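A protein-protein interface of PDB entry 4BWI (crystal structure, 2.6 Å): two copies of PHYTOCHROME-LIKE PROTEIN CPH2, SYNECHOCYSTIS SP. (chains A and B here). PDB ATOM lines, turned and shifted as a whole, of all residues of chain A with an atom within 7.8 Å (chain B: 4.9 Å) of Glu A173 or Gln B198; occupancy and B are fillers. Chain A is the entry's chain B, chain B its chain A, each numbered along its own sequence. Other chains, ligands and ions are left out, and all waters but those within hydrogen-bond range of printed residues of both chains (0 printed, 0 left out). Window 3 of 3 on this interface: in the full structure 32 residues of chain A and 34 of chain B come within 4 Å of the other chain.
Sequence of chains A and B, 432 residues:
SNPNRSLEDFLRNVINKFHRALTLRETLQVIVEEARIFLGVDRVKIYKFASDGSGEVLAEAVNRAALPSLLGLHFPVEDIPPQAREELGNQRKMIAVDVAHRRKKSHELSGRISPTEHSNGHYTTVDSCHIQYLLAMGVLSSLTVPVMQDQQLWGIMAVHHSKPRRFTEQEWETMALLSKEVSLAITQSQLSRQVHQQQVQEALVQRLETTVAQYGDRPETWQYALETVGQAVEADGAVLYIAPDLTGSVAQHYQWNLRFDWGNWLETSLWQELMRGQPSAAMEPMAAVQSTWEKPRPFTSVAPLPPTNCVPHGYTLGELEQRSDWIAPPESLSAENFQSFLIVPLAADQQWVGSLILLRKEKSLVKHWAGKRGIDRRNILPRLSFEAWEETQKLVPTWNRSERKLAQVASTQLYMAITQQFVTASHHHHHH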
ATOM      1  N   PHE A  38     -11.446  -8.200  30.672  1.00  0.00           N
ATOM      2  CA  PHE A  38     -11.520  -9.635  30.930  1.00  0.00           C
ATOM      3  C   PHE A  38     -10.437 -10.422  30.193  1.00  0.00           C
ATOM      4  O   PHE A  38      -9.844 -11.343  30.751  1.00  0.00           O
ATOM      5  CB  PHE A  38     -12.907 -10.174  30.562  1.00  0.00           C
ATOM      6  CG  PHE A  38     -12.983 -11.672  30.530  1.00  0.00           C
ATOM      7  CD1 PHE A  38     -12.925 -12.407  31.704  1.00  0.00           C
ATOM      8  CD2 PHE A  38     -13.114 -12.347  29.327  1.00  0.00           C
ATOM      9  CE1 PHE A  38     -12.994 -13.786  31.678  1.00  0.00           C
ATOM     10  CE2 PHE A  38     -13.184 -13.726  29.295  1.00  0.00           C
ATOM     11  CZ  PHE A  38     -13.123 -14.446  30.471  1.00  0.00           C
ATOM     12  N   MET A  94     -16.391 -17.801  14.176  1.00  0.00           N
ATOM     13  CA  MET A  94     -15.457 -16.933  14.874  1.00  0.00           C
ATOM     14  C   MET A  94     -14.066 -17.284  14.359  1.00  0.00           C
ATOM     15  O   MET A  94     -13.664 -18.447  14.388  1.00  0.00           O
ATOM     16  CB  MET A  94     -15.535 -17.155  16.384  1.00  0.00           C
ATOM     17  CG  MET A  94     -16.879 -16.799  17.000  1.00  0.00           C
ATOM     18  SD  MET A  94     -16.997 -17.309  18.727  1.00  0.00           S
ATOM     19  CE  MET A  94     -15.596 -16.447  19.432  1.00  0.00           C
ATOM     20  N   HIS A 107     -14.114 -21.364  14.791  1.00  0.00           N
ATOM     21  CA  HIS A 107     -15.043 -22.049  15.682  1.00  0.00           C
ATOM     22  C   HIS A 107     -16.460 -21.518  15.502  1.00  0.00           C
ATOM     23  O   HIS A 107     -16.660 -20.333  15.229  1.00  0.00           O
ATOM     24  CB  HIS A 107     -14.602 -21.912  17.141  1.00  0.00           C
ATOM     25  CG  HIS A 107     -13.547 -22.895  17.549  1.00  0.00           C
ATOM     26  ND1 HIS A 107     -12.684 -22.667  18.600  1.00  0.00           N
ATOM     27  CD2 HIS A 107     -13.223 -24.113  17.055  1.00  0.00           C
ATOM     28  CE1 HIS A 107     -11.870 -23.699  18.730  1.00  0.00           C
ATOM     29  NE2 HIS A 107     -12.177 -24.591  17.805  1.00  0.00           N
ATOM     30  N   GLU A 108     -17.439 -22.405  15.649  1.00  0.00           N
ATOM     31  CA  GLU A 108     -18.844 -22.038  15.507  1.00  0.00           C
ATOM     32  C   GLU A 108     -19.296 -21.086  16.610  1.00  0.00           C
ATOM     33  O   GLU A 108     -18.949 -21.262  17.777  1.00  0.00           O
ATOM     34  CB  GLU A 108     -19.723 -23.291  15.498  1.00  0.00           C
ATOM     35  CG  GLU A 108     -19.808 -23.979  14.146  1.00  0.00           C
ATOM     36  CD  GLU A 108     -20.660 -23.208  13.157  1.00  0.00           C
ATOM     37  OE1 GLU A 108     -21.518 -22.418  13.601  1.00  0.00           O
ATOM     38  OE2 GLU A 108     -20.472 -23.394  11.935  1.00  0.00           O
ATOM     39  N   LEU A 109     -20.080 -20.083  16.226  1.00  0.00           N
ATOM     40  CA  LEU A 109     -20.586 -19.083  17.160  1.00  0.00           C
ATOM     41  C   LEU A 109     -21.470 -19.700  18.246  1.00  0.00           C
ATOM     42  O   LEU A 109     -21.601 -19.149  19.339  1.00  0.00           O
ATOM     43  CB  LEU A 109     -21.361 -18.003  16.400  1.00  0.00           C
ATOM     44  CG  LEU A 109     -21.842 -16.770  17.167  1.00  0.00           C
ATOM     45  CD1 LEU A 109     -20.662 -15.961  17.691  1.00  0.00           C
ATOM     46  CD2 LEU A 109     -22.731 -15.916  16.277  1.00  0.00           C
ATOM     47  N   SER A 110     -22.073 -20.846  17.945  1.00  0.00           N
ATOM     48  CA  SER A 110     -22.946 -21.522  18.899  1.00  0.00           C
ATOM     49  C   SER A 110     -22.429 -22.908  19.281  1.00  0.00           C
ATOM     50  O   SER A 110     -22.878 -23.496  20.265  1.00  0.00           O
ATOM     51  CB  SER A 110     -24.367 -21.623  18.343  1.00  0.00           C
ATOM     52  OG  SER A 110     -24.910 -20.336  18.106  1.00  0.00           O
ATOM     53  N   GLY A 111     -21.486 -23.424  18.498  1.00  0.00           N
ATOM     54  CA  GLY A 111     -20.914 -24.736  18.753  1.00  0.00           C
ATOM     55  C   GLY A 111     -19.916 -24.732  19.895  1.00  0.00           C
ATOM     56  O   GLY A 111     -19.032 -23.875  19.951  1.00  0.00           O
ATOM     57  N   ARG A 112     -20.053 -25.698  20.800  1.00  0.00           N
ATOM     58  CA  ARG A 112     -19.193 -25.788  21.979  1.00  0.00           C
ATOM     59  C   ARG A 112     -19.343 -27.125  22.707  1.00  0.00           C
ATOM     60  O   ARG A 112     -20.437 -27.489  23.139  1.00  0.00           O
ATOM     61  CB  ARG A 112     -19.496 -24.639  22.944  1.00  0.00           C
ATOM     62  CG  ARG A 112     -19.040 -24.886  24.373  1.00  0.00           C
ATOM     63  CD  ARG A 112     -20.113 -24.477  25.375  1.00  0.00           C
ATOM     64  NE  ARG A 112     -21.341 -25.253  25.222  1.00  0.00           N
ATOM     65  CZ  ARG A 112     -22.424 -24.828  24.579  1.00  0.00           C
ATOM     66  NH1 ARG A 112     -22.438 -23.623  24.024  1.00  0.00           N
ATOM     67  NH2 ARG A 112     -23.494 -25.606  24.489  1.00  0.00           N
ATOM     68  N   ILE A 113     -18.235 -27.850  22.839  1.00  0.00           N
ATOM     69  CA  ILE A 113     -18.209 -29.102  23.593  1.00  0.00           C
ATOM     70  C   ILE A 113     -16.916 -29.231  24.395  1.00  0.00           C
ATOM     71  O   ILE A 113     -15.863 -28.741  23.982  1.00  0.00           O
ATOM     72  CB  ILE A 113     -18.363 -30.337  22.679  1.00  0.00           C
ATOM     73  CG1 ILE A 113     -19.818 -30.501  22.236  1.00  0.00           C
ATOM     74  CG2 ILE A 113     -17.893 -31.594  23.397  1.00  0.00           C
ATOM     75  CD1 ILE A 113     -20.065 -31.717  21.369  1.00  0.00           C
ATOM     76  N   LEU A 143      -8.980 -11.908  16.981  1.00  0.00           N
ATOM     77  CA  LEU A 143     -10.191 -12.720  17.068  1.00  0.00           C
ATOM     78  C   LEU A 143     -11.388 -11.943  16.524  1.00  0.00           C
ATOM     79  O   LEU A 143     -11.767 -10.904  17.067  1.00  0.00           O
ATOM     80  CB  LEU A 143     -10.466 -13.167  18.504  1.00  0.00           C
ATOM     81  CG  LEU A 143     -11.726 -14.029  18.644  1.00  0.00           C
ATOM     82  CD1 LEU A 143     -11.554 -15.353  17.908  1.00  0.00           C
ATOM     83  CD2 LEU A 143     -12.085 -14.264  20.105  1.00  0.00           C
ATOM     84  N   THR A 168      -8.186 -19.255  25.040  1.00  0.00           N
ATOM     85  CA  THR A 168      -8.692 -20.491  25.626  1.00  0.00           C
ATOM     86  C   THR A 168     -10.163 -20.669  25.289  1.00  0.00           C
ATOM     87  O   THR A 168     -10.845 -19.706  24.941  1.00  0.00           O
ATOM     88  CB  THR A 168      -8.542 -20.497  27.155  1.00  0.00           C
ATOM     89  OG1 THR A 168      -9.336 -19.445  27.717  1.00  0.00           O
ATOM     90  CG2 THR A 168      -7.086 -20.301  27.551  1.00  0.00           C
ATOM     91  N   GLU A 169     -10.646 -21.903  25.404  1.00  0.00           N
ATOM     92  CA  GLU A 169     -12.038 -22.224  25.105  1.00  0.00           C
ATOM     93  C   GLU A 169     -12.999 -21.354  25.910  1.00  0.00           C
ATOM     94  O   GLU A 169     -14.023 -20.906  25.393  1.00  0.00           O
ATOM     95  CB  GLU A 169     -12.313 -23.704  25.378  1.00  0.00           C
ATOM     96  CG  GLU A 169     -13.725 -24.153  25.038  1.00  0.00           C
ATOM     97  CD  GLU A 169     -13.980 -25.607  25.393  1.00  0.00           C
ATOM     98  OE1 GLU A 169     -13.080 -26.246  25.976  1.00  0.00           O
ATOM     99  OE2 GLU A 169     -15.081 -26.109  25.086  1.00  0.00           O
ATOM    100  N   GLN A 170     -12.654 -21.108  27.171  1.00  0.00           N
ATOM    101  CA  GLN A 170     -13.472 -20.282  28.054  1.00  0.00           C
ATOM    102  C   GLN A 170     -13.656 -18.871  27.500  1.00  0.00           C
ATOM    103  O   GLN A 170     -14.686 -18.235  27.727  1.00  0.00           O
ATOM    104  CB  GLN A 170     -12.854 -20.205  29.454  1.00  0.00           C
ATOM    105  CG  GLN A 170     -12.768 -21.536  30.192  1.00  0.00           C
ATOM    106  CD  GLN A 170     -11.514 -22.326  29.852  1.00  0.00           C
ATOM    107  OE1 GLN A 170     -10.915 -22.144  28.792  1.00  0.00           O
ATOM    108  NE2 GLN A 170     -11.108 -23.205  30.761  1.00  0.00           N
ATOM    109  N   GLU A 171     -12.652 -18.394  26.771  1.00  0.00           N
ATOM    110  CA  GLU A 171     -12.680 -17.048  26.212  1.00  0.00           C
ATOM    111  C   GLU A 171     -13.478 -16.977  24.912  1.00  0.00           C
ATOM    112  O   GLU A 171     -14.113 -15.963  24.625  1.00  0.00           O
ATOM    113  CB  GLU A 171     -11.257 -16.535  25.999  1.00  0.00           C
ATOM    114  CG  GLU A 171     -10.476 -16.374  27.290  1.00  0.00           C
ATOM    115  CD  GLU A 171      -9.009 -16.071  27.058  1.00  0.00           C
ATOM    116  OE1 GLU A 171      -8.466 -16.487  26.010  1.00  0.00           O
ATOM    117  OE2 GLU A 171      -8.395 -15.423  27.933  1.00  0.00           O
ATOM    118  N   TRP A 172     -13.441 -18.053  24.132  1.00  0.00           N
ATOM    119  CA  TRP A 172     -14.223 -18.135  22.901  1.00  0.00           C
ATOM    120  C   TRP A 172     -15.714 -18.051  23.209  1.00  0.00           C
ATOM    121  O   TRP A 172     -16.434 -17.247  22.616  1.00  0.00           O
ATOM    122  CB  TRP A 172     -13.934 -19.442  22.161  1.00  0.00           C
ATOM    123  CG  TRP A 172     -12.603 -19.486  21.479  1.00  0.00           C
ATOM    124  CD1 TRP A 172     -11.386 -19.668  22.066  1.00  0.00           C
ATOM    125  CD2 TRP A 172     -12.357 -19.369  20.074  1.00  0.00           C
ATOM    126  NE1 TRP A 172     -10.399 -19.662  21.118  1.00  0.00           N
ATOM    127  CE2 TRP A 172     -10.967 -19.480  19.885  1.00  0.00           C
ATOM    128  CE3 TRP A 172     -13.176 -19.176  18.959  1.00  0.00           C
ATOM    129  CZ2 TRP A 172     -10.377 -19.405  18.626  1.00  0.00           C
ATOM    130  CZ3 TRP A 172     -12.589 -19.103  17.709  1.00  0.00           C
ATOM    131  CH2 TRP A 172     -11.203 -19.218  17.553  1.00  0.00           C
ATOM    132  N   GLU A 173     -16.165 -18.892  24.137  1.00  0.00           N
ATOM    133  CA  GLU A 173     -17.561 -18.920  24.553  1.00  0.00           C
ATOM    134  C   GLU A 173     -17.993 -17.563  25.088  1.00  0.00           C
ATOM    135  O   GLU A 173     -19.090 -17.089  24.803  1.00  0.00           O
ATOM    136  CB  GLU A 173     -17.775 -19.984  25.632  1.00  0.00           C
ATOM    137  CG  GLU A 173     -17.378 -21.389  25.221  1.00  0.00           C
ATOM    138  CD  GLU A 173     -17.528 -22.387  26.354  1.00  0.00           C
ATOM    139  OE1 GLU A 173     -18.317 -22.116  27.285  1.00  0.00           O
ATOM    140  OE2 GLU A 173     -16.853 -23.438  26.317  1.00  0.00           O
ATOM    141  N   THR A 174     -17.112 -16.946  25.867  1.00  0.00           N
ATOM    142  CA  THR A 174     -17.393 -15.655  26.477  1.00  0.00           C
ATOM    143  C   THR A 174     -17.624 -14.578  25.418  1.00  0.00           C
ATOM    144  O   THR A 174     -18.542 -13.768  25.538  1.00  0.00           O
ATOM    145  CB  THR A 174     -16.251 -15.234  27.419  1.00  0.00           C
ATOM    146  OG1 THR A 174     -16.055 -16.249  28.411  1.00  0.00           O
ATOM    147  CG2 THR A 174     -16.579 -13.925  28.104  1.00  0.00           C
ATOM    148  N   MET A 175     -16.796 -14.577  24.378  1.00  0.00           N
ATOM    149  CA  MET A 175     -16.954 -13.617  23.290  1.00  0.00           C
ATOM    150  C   MET A 175     -18.215 -13.907  22.484  1.00  0.00           C
ATOM    151  O   MET A 175     -18.918 -12.988  22.067  1.00  0.00           O
ATOM    152  CB  MET A 175     -15.725 -13.619  22.373  1.00  0.00           C
ATOM    153  CG  MET A 175     -14.440 -13.192  23.056  1.00  0.00           C
ATOM    154  SD  MET A 175     -14.630 -11.662  23.991  1.00  0.00           S
ATOM    155  CE  MET A 175     -15.073 -10.519  22.687  1.00  0.00           C
ATOM    156  N   ALA A 176     -18.488 -15.190  22.268  1.00  0.00           N
ATOM    157  CA  ALA A 176     -19.710 -15.619  21.595  1.00  0.00           C
ATOM    158  C   ALA A 176     -20.933 -15.116  22.353  1.00  0.00           C
ATOM    159  O   ALA A 176     -21.901 -14.644  21.756  1.00  0.00           O
ATOM    160  CB  ALA A 176     -19.743 -17.133  21.482  1.00  0.00           C
ATOM    161  N   LEU A 177     -20.867 -15.214  23.677  1.00  0.00           N
ATOM    162  CA  LEU A 177     -21.926 -14.741  24.557  1.00  0.00           C
ATOM    163  C   LEU A 177     -22.108 -13.228  24.434  1.00  0.00           C
ATOM    164  O   LEU A 177     -23.236 -12.729  24.409  1.00  0.00           O
ATOM    165  CB  LEU A 177     -21.616 -15.137  26.004  1.00  0.00           C
ATOM    166  CG  LEU A 177     -22.700 -14.977  27.071  1.00  0.00           C
ATOM    167  CD1 LEU A 177     -22.604 -16.111  28.076  1.00  0.00           C
ATOM    168  CD2 LEU A 177     -22.572 -13.636  27.776  1.00  0.00           C
ATOM    169  N   LEU A 178     -20.997 -12.501  24.354  1.00  0.00           N
ATOM    170  CA  LEU A 178     -21.049 -11.049  24.207  1.00  0.00           C
ATOM    171  C   LEU A 178     -21.599 -10.646  22.846  1.00  0.00           C
ATOM    172  O   LEU A 178     -22.232  -9.602  22.708  1.00  0.00           O
ATOM    173  CB  LEU A 178     -19.670 -10.423  24.420  1.00  0.00           C
ATOM    174  CG  LEU A 178     -19.170 -10.371  25.862  1.00  0.00           C
ATOM    175  CD1 LEU A 178     -17.888  -9.563  25.935  1.00  0.00           C
ATOM    176  CD2 LEU A 178     -20.237  -9.781  26.769  1.00  0.00           C
ATOM    177  N   SER A 179     -21.357 -11.476  21.840  1.00  0.00           N
ATOM    178  CA  SER A 179     -21.919 -11.233  20.519  1.00  0.00           C
ATOM    179  C   SER A 179     -23.440 -11.367  20.553  1.00  0.00           C
ATOM    180  O   SER A 179     -24.154 -10.613  19.893  1.00  0.00           O
ATOM    181  CB  SER A 179     -21.321 -12.187  19.489  1.00  0.00           C
ATOM    182  OG  SER A 179     -21.886 -11.964  18.211  1.00  0.00           O
ATOM    183  N   LYS A 180     -23.934 -12.332  21.323  1.00  0.00           N
ATOM    184  CA  LYS A 180     -25.373 -12.489  21.495  1.00  0.00           C
ATOM    185  C   LYS A 180     -25.943 -11.320  22.295  1.00  0.00           C
ATOM    186  O   LYS A 180     -27.064 -10.883  22.050  1.00  0.00           O
ATOM    187  CB  LYS A 180     -25.706 -13.825  22.162  1.00  0.00           C
ATOM    188  CG  LYS A 180     -25.388 -15.038  21.296  1.00  0.00           C
ATOM    189  CD  LYS A 180     -25.891 -16.324  21.933  1.00  0.00           C
ATOM    190  CE  LYS A 180     -25.582 -17.532  21.065  1.00  0.00           C
ATOM    191  NZ  LYS A 180     -26.193 -17.415  19.712  1.00  0.00           N
ATOM    192  N   LEU B   7     -13.478 -15.053  35.490  1.00  0.00           N
ATOM    193  CA  LEU B   7     -14.710 -15.331  34.760  1.00  0.00           C
ATOM    194  C   LEU B   7     -15.928 -15.151  35.658  1.00  0.00           C
ATOM    195  O   LEU B   7     -16.956 -14.631  35.228  1.00  0.00           O
ATOM    196  CB  LEU B   7     -14.684 -16.751  34.191  1.00  0.00           C
ATOM    197  CG  LEU B   7     -15.907 -17.186  33.381  1.00  0.00           C
ATOM    198  CD1 LEU B   7     -16.077 -16.310  32.148  1.00  0.00           C
ATOM    199  CD2 LEU B   7     -15.804 -18.655  32.995  1.00  0.00           C
ATOM    200  N   LEU B  11     -19.110 -12.754  34.564  1.00  0.00           N
ATOM    201  CA  LEU B  11     -20.452 -13.243  34.268  1.00  0.00           C
ATOM    202  C   LEU B  11     -21.484 -12.539  35.141  1.00  0.00           C
ATOM    203  O   LEU B  11     -22.628 -12.338  34.731  1.00  0.00           O
ATOM    204  CB  LEU B  11     -20.525 -14.757  34.473  1.00  0.00           C
ATOM    205  CG  LEU B  11     -19.597 -15.593  33.589  1.00  0.00           C
ATOM    206  CD1 LEU B  11     -19.610 -17.047  34.025  1.00  0.00           C
ATOM    207  CD2 LEU B  11     -19.988 -15.461  32.124  1.00  0.00           C
ATOM    208  N   GLN B 194     -28.366 -18.838  29.535  1.00  0.00           N
ATOM    209  CA  GLN B 194     -27.052 -19.307  29.110  1.00  0.00           C
ATOM    210  C   GLN B 194     -25.932 -18.697  29.948  1.00  0.00           C
ATOM    211  O   GLN B 194     -24.941 -19.365  30.248  1.00  0.00           O
ATOM    212  CB  GLN B 194     -26.829 -19.035  27.621  1.00  0.00           C
ATOM    213  CG  GLN B 194     -27.713 -19.876  26.714  1.00  0.00           C
ATOM    214  CD  GLN B 194     -27.496 -19.592  25.241  1.00  0.00           C
ATOM    215  OE1 GLN B 194     -27.003 -18.527  24.866  1.00  0.00           O
ATOM    216  NE2 GLN B 194     -27.863 -20.548  24.397  1.00  0.00           N
ATOM    217  N   VAL B 195     -26.095 -17.434  30.329  1.00  0.00           N
ATOM    218  CA  VAL B 195     -25.131 -16.783  31.206  1.00  0.00           C
ATOM    219  C   VAL B 195     -25.130 -17.459  32.571  1.00  0.00           C
ATOM    220  O   VAL B 195     -24.074 -17.755  33.129  1.00  0.00           O
ATOM    221  CB  VAL B 195     -25.428 -15.280  31.377  1.00  0.00           C
ATOM    222  CG1 VAL B 195     -24.428 -14.647  32.333  1.00  0.00           C
ATOM    223  CG2 VAL B 195     -25.393 -14.581  30.031  1.00  0.00           C
ATOM    224  N   HIS B 196     -26.324 -17.709  33.098  1.00  0.00           N
ATOM    225  CA  HIS B 196     -26.476 -18.350  34.398  1.00  0.00           C
ATOM    226  C   HIS B 196     -25.884 -19.759  34.422  1.00  0.00           C
ATOM    227  O   HIS B 196     -25.374 -20.210  35.449  1.00  0.00           O
ATOM    228  CB  HIS B 196     -27.950 -18.398  34.802  1.00  0.00           C
ATOM    229  CG  HIS B 196     -28.195 -19.091  36.105  1.00  0.00           C
ATOM    230  ND1 HIS B 196     -28.022 -18.468  37.322  1.00  0.00           N
ATOM    231  CD2 HIS B 196     -28.585 -20.357  36.383  1.00  0.00           C
ATOM    232  CE1 HIS B 196     -28.303 -19.318  38.293  1.00  0.00           C
ATOM    233  NE2 HIS B 196     -28.647 -20.473  37.750  1.00  0.00           N
ATOM    234  N   GLN B 197     -25.956 -20.454  33.293  1.00  0.00           N
ATOM    235  CA  GLN B 197     -25.375 -21.787  33.191  1.00  0.00           C
ATOM    236  C   GLN B 197     -23.851 -21.711  33.196  1.00  0.00           C
ATOM    237  O   GLN B 197     -23.174 -22.637  33.642  1.00  0.00           O
ATOM    238  CB  GLN B 197     -25.883 -22.505  31.939  1.00  0.00           C
ATOM    239  CG  GLN B 197     -27.360 -22.876  31.998  1.00  0.00           C
ATOM    240  CD  GLN B 197     -27.878 -23.450  30.692  1.00  0.00           C
ATOM    241  OE1 GLN B 197     -27.143 -23.560  29.710  1.00  0.00           O
ATOM    242  NE2 GLN B 197     -29.154 -23.820  30.674  1.00  0.00           N
ATOM    243  N   GLN B 198     -23.320 -20.598  32.700  1.00  0.00           N
ATOM    244  CA  GLN B 198     -21.884 -20.350  32.730  1.00  0.00           C
ATOM    245  C   GLN B 198     -21.412 -20.065  34.155  1.00  0.00           C
ATOM    246  O   GLN B 198     -20.295 -20.415  34.531  1.00  0.00           O
ATOM    247  CB  GLN B 198     -21.523 -19.186  31.804  1.00  0.00           C
ATOM    248  CG  GLN B 198     -21.152 -19.594  30.387  1.00  0.00           C
ATOM    249  CD  GLN B 198     -19.667 -19.421  30.110  1.00  0.00           C
ATOM    250  OE1 GLN B 198     -18.909 -20.393  30.089  1.00  0.00           O
ATOM    251  NE2 GLN B 198     -19.246 -18.177  29.898  1.00  0.00           N
ATOM    252  N   GLN B 199     -22.274 -19.429  34.944  1.00  0.00           N
ATOM    253  CA  GLN B 199     -21.972 -19.150  36.344  1.00  0.00           C
ATOM    254  C   GLN B 199     -21.951 -20.431  37.169  1.00  0.00           C
ATOM    255  O   GLN B 199     -21.084 -20.616  38.018  1.00  0.00           O
ATOM    256  CB  GLN B 199     -22.995 -18.180  36.932  1.00  0.00           C
ATOM    257  CG  GLN B 199     -22.915 -16.773  36.373  1.00  0.00           C
ATOM    258  CD  GLN B 199     -24.088 -15.918  36.804  1.00  0.00           C
ATOM    259  OE1 GLN B 199     -25.233 -16.372  36.808  1.00  0.00           O
ATOM    260  NE2 GLN B 199     -23.809 -14.675  37.177  1.00  0.00           N
ATOM    261  N   VAL B 200     -22.916 -21.306  36.915  1.00  0.00           N
ATOM    262  CA  VAL B 200     -23.009 -22.584  37.614  1.00  0.00           C
ATOM    263  C   VAL B 200     -21.810 -23.463  37.276  1.00  0.00           C
ATOM    264  O   VAL B 200     -21.262 -24.155  38.137  1.00  0.00           O
ATOM    265  CB  VAL B 200     -24.323 -23.312  37.253  1.00  0.00           C
ATOM    266  CG1 VAL B 200     -24.298 -24.756  37.728  1.00  0.00           C
ATOM    267  CG2 VAL B 200     -25.513 -22.566  37.841  1.00  0.00           C
ATOM    268  N   GLN B 201     -21.400 -23.414  36.015  1.00  0.00           N
ATOM    269  CA  GLN B 201     -20.244 -24.161  35.543  1.00  0.00           C
ATOM    270  C   GLN B 201     -18.978 -23.720  36.274  1.00  0.00           C
ATOM    271  O   GLN B 201     -18.223 -24.547  36.788  1.00  0.00           O
ATOM    272  CB  GLN B 201     -20.083 -23.962  34.036  1.00  0.00           C
ATOM    273  CG  GLN B 201     -19.231 -25.004  33.345  1.00  0.00           C
ATOM    274  CD  GLN B 201     -19.261 -24.857  31.835  1.00  0.00           C
ATOM    275  OE1 GLN B 201     -19.443 -25.832  31.107  1.00  0.00           O
ATOM    276  NE2 GLN B 201     -19.084 -23.630  31.358  1.00  0.00           N
ATOM    277  N   GLU B 202     -18.760 -22.410  36.328  1.00  0.00           N
ATOM    278  CA  GLU B 202     -17.568 -21.851  36.958  1.00  0.00           C
ATOM    279  C   GLU B 202     -17.588 -22.022  38.477  1.00  0.00           C
ATOM    280  O   GLU B 202     -16.549 -22.270  39.093  1.00  0.00           O
ATOM    281  CB  GLU B 202     -17.403 -20.373  36.580  1.00  0.00           C
ATOM    282  CG  GLU B 202     -16.256 -19.662  37.282  1.00  0.00           C
ATOM    283  CD  GLU B 202     -14.887 -20.179  36.867  1.00  0.00           C
ATOM    284  OE1 GLU B 202     -14.791 -20.868  35.828  1.00  0.00           O
ATOM    285  OE2 GLU B 202     -13.903 -19.892  37.584  1.00  0.00           O
ATOM    286  N   LYS B 405     -22.673 -30.840  29.379  1.00  0.00           N
ATOM    287  CA  LYS B 405     -21.496 -29.981  29.369  1.00  0.00           C
ATOM    288  C   LYS B 405     -20.947 -29.859  30.784  1.00  0.00           C
ATOM    289  O   LYS B 405     -19.736 -29.919  31.000  1.00  0.00           O
ATOM    290  CB  LYS B 405     -21.849 -28.595  28.829  1.00  0.00           C
ATOM    291  CG  LYS B 405     -20.853 -28.036  27.822  1.00  0.00           C
ATOM    292  CD  LYS B 405     -19.465 -27.875  28.420  1.00  0.00           C
ATOM    293  CE  LYS B 405     -18.489 -27.326  27.392  1.00  0.00           C
ATOM    294  NZ  LYS B 405     -17.114 -27.189  27.947  1.00  0.00           N
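NZ of Lys B405 lies within salt-bridge range of OE2 of Glu A169, 3.7 Å away. The side-chain amide oxygen of Gln B198 sits close to the side-chain carboxylate of Glu A173 (3.3 Å).
O of Gln A170 is in hydrogen-bond range of OG1 of Thr A174, at 2.5 Å. The side-chain amide oxygen (OE1) of Gln B198 is in hydrogen-bond range of the side-chain amide nitrogen (NE2) of Gln B201 (3.5 Å).
CE1 of Phe A38 touches CA of Leu B7 (3.9 Å). Lys B405 touches Arg A112 (CG to NE, 3.8 Å). CE of Lys B405 touches C of Ile A113 (3.9 Å). CD1 of Leu B7 touches OG1 of Thr A174, at 3.7 Å. Leu A177 touches Val B195 (CD2 to CG2, 3.7 Å). Lys A180 touches Gln B194.
Printed residues of chain B within 4 Å of Thr A174: Leu B7 (3.7 Å). Printed residues of chain A within 4 Å of Gln B194: Lys A180 (3.8 Å). Printed residues of chain A within 4 Å of Val B195: Leu A177. Printed residues of chain A within 4 Å of Gln B198: Glu A173. The nearest residue of chain B that does not touch Glu A173 is Lys B405 (4.1 Å).
Printed residues of chain A that touch a printed residue of chain B: Phe A38, Arg A112, Ile A113, Glu A169, Glu A173, Thr A174, Leu A177 and Lys A180. Hydrophobic or aromatic side chains of chain A that line the printed part of chain B: Phe A38 and Leu A177. Of the 12 printed residues of chain B, 5 touch a printed residue of chain A. Printed residues of chain B that touch a printed residue of chain A: Leu B7, Gln B194, Val B195, Gln B198 and Lys B405. Among the printed residues, 8 pairs touch across the chains. Among the printed residues, Asp or Glu carboxylates within 4 Å of a Lys or Arg side-chain nitrogen of the other chain: Glu A169 with Lys B405 (3.7 Å).
No position is printed for both chains. Of the 8 pairs that touch across the chains among the printed residues, none has its exchanged pair printed and touching as well.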
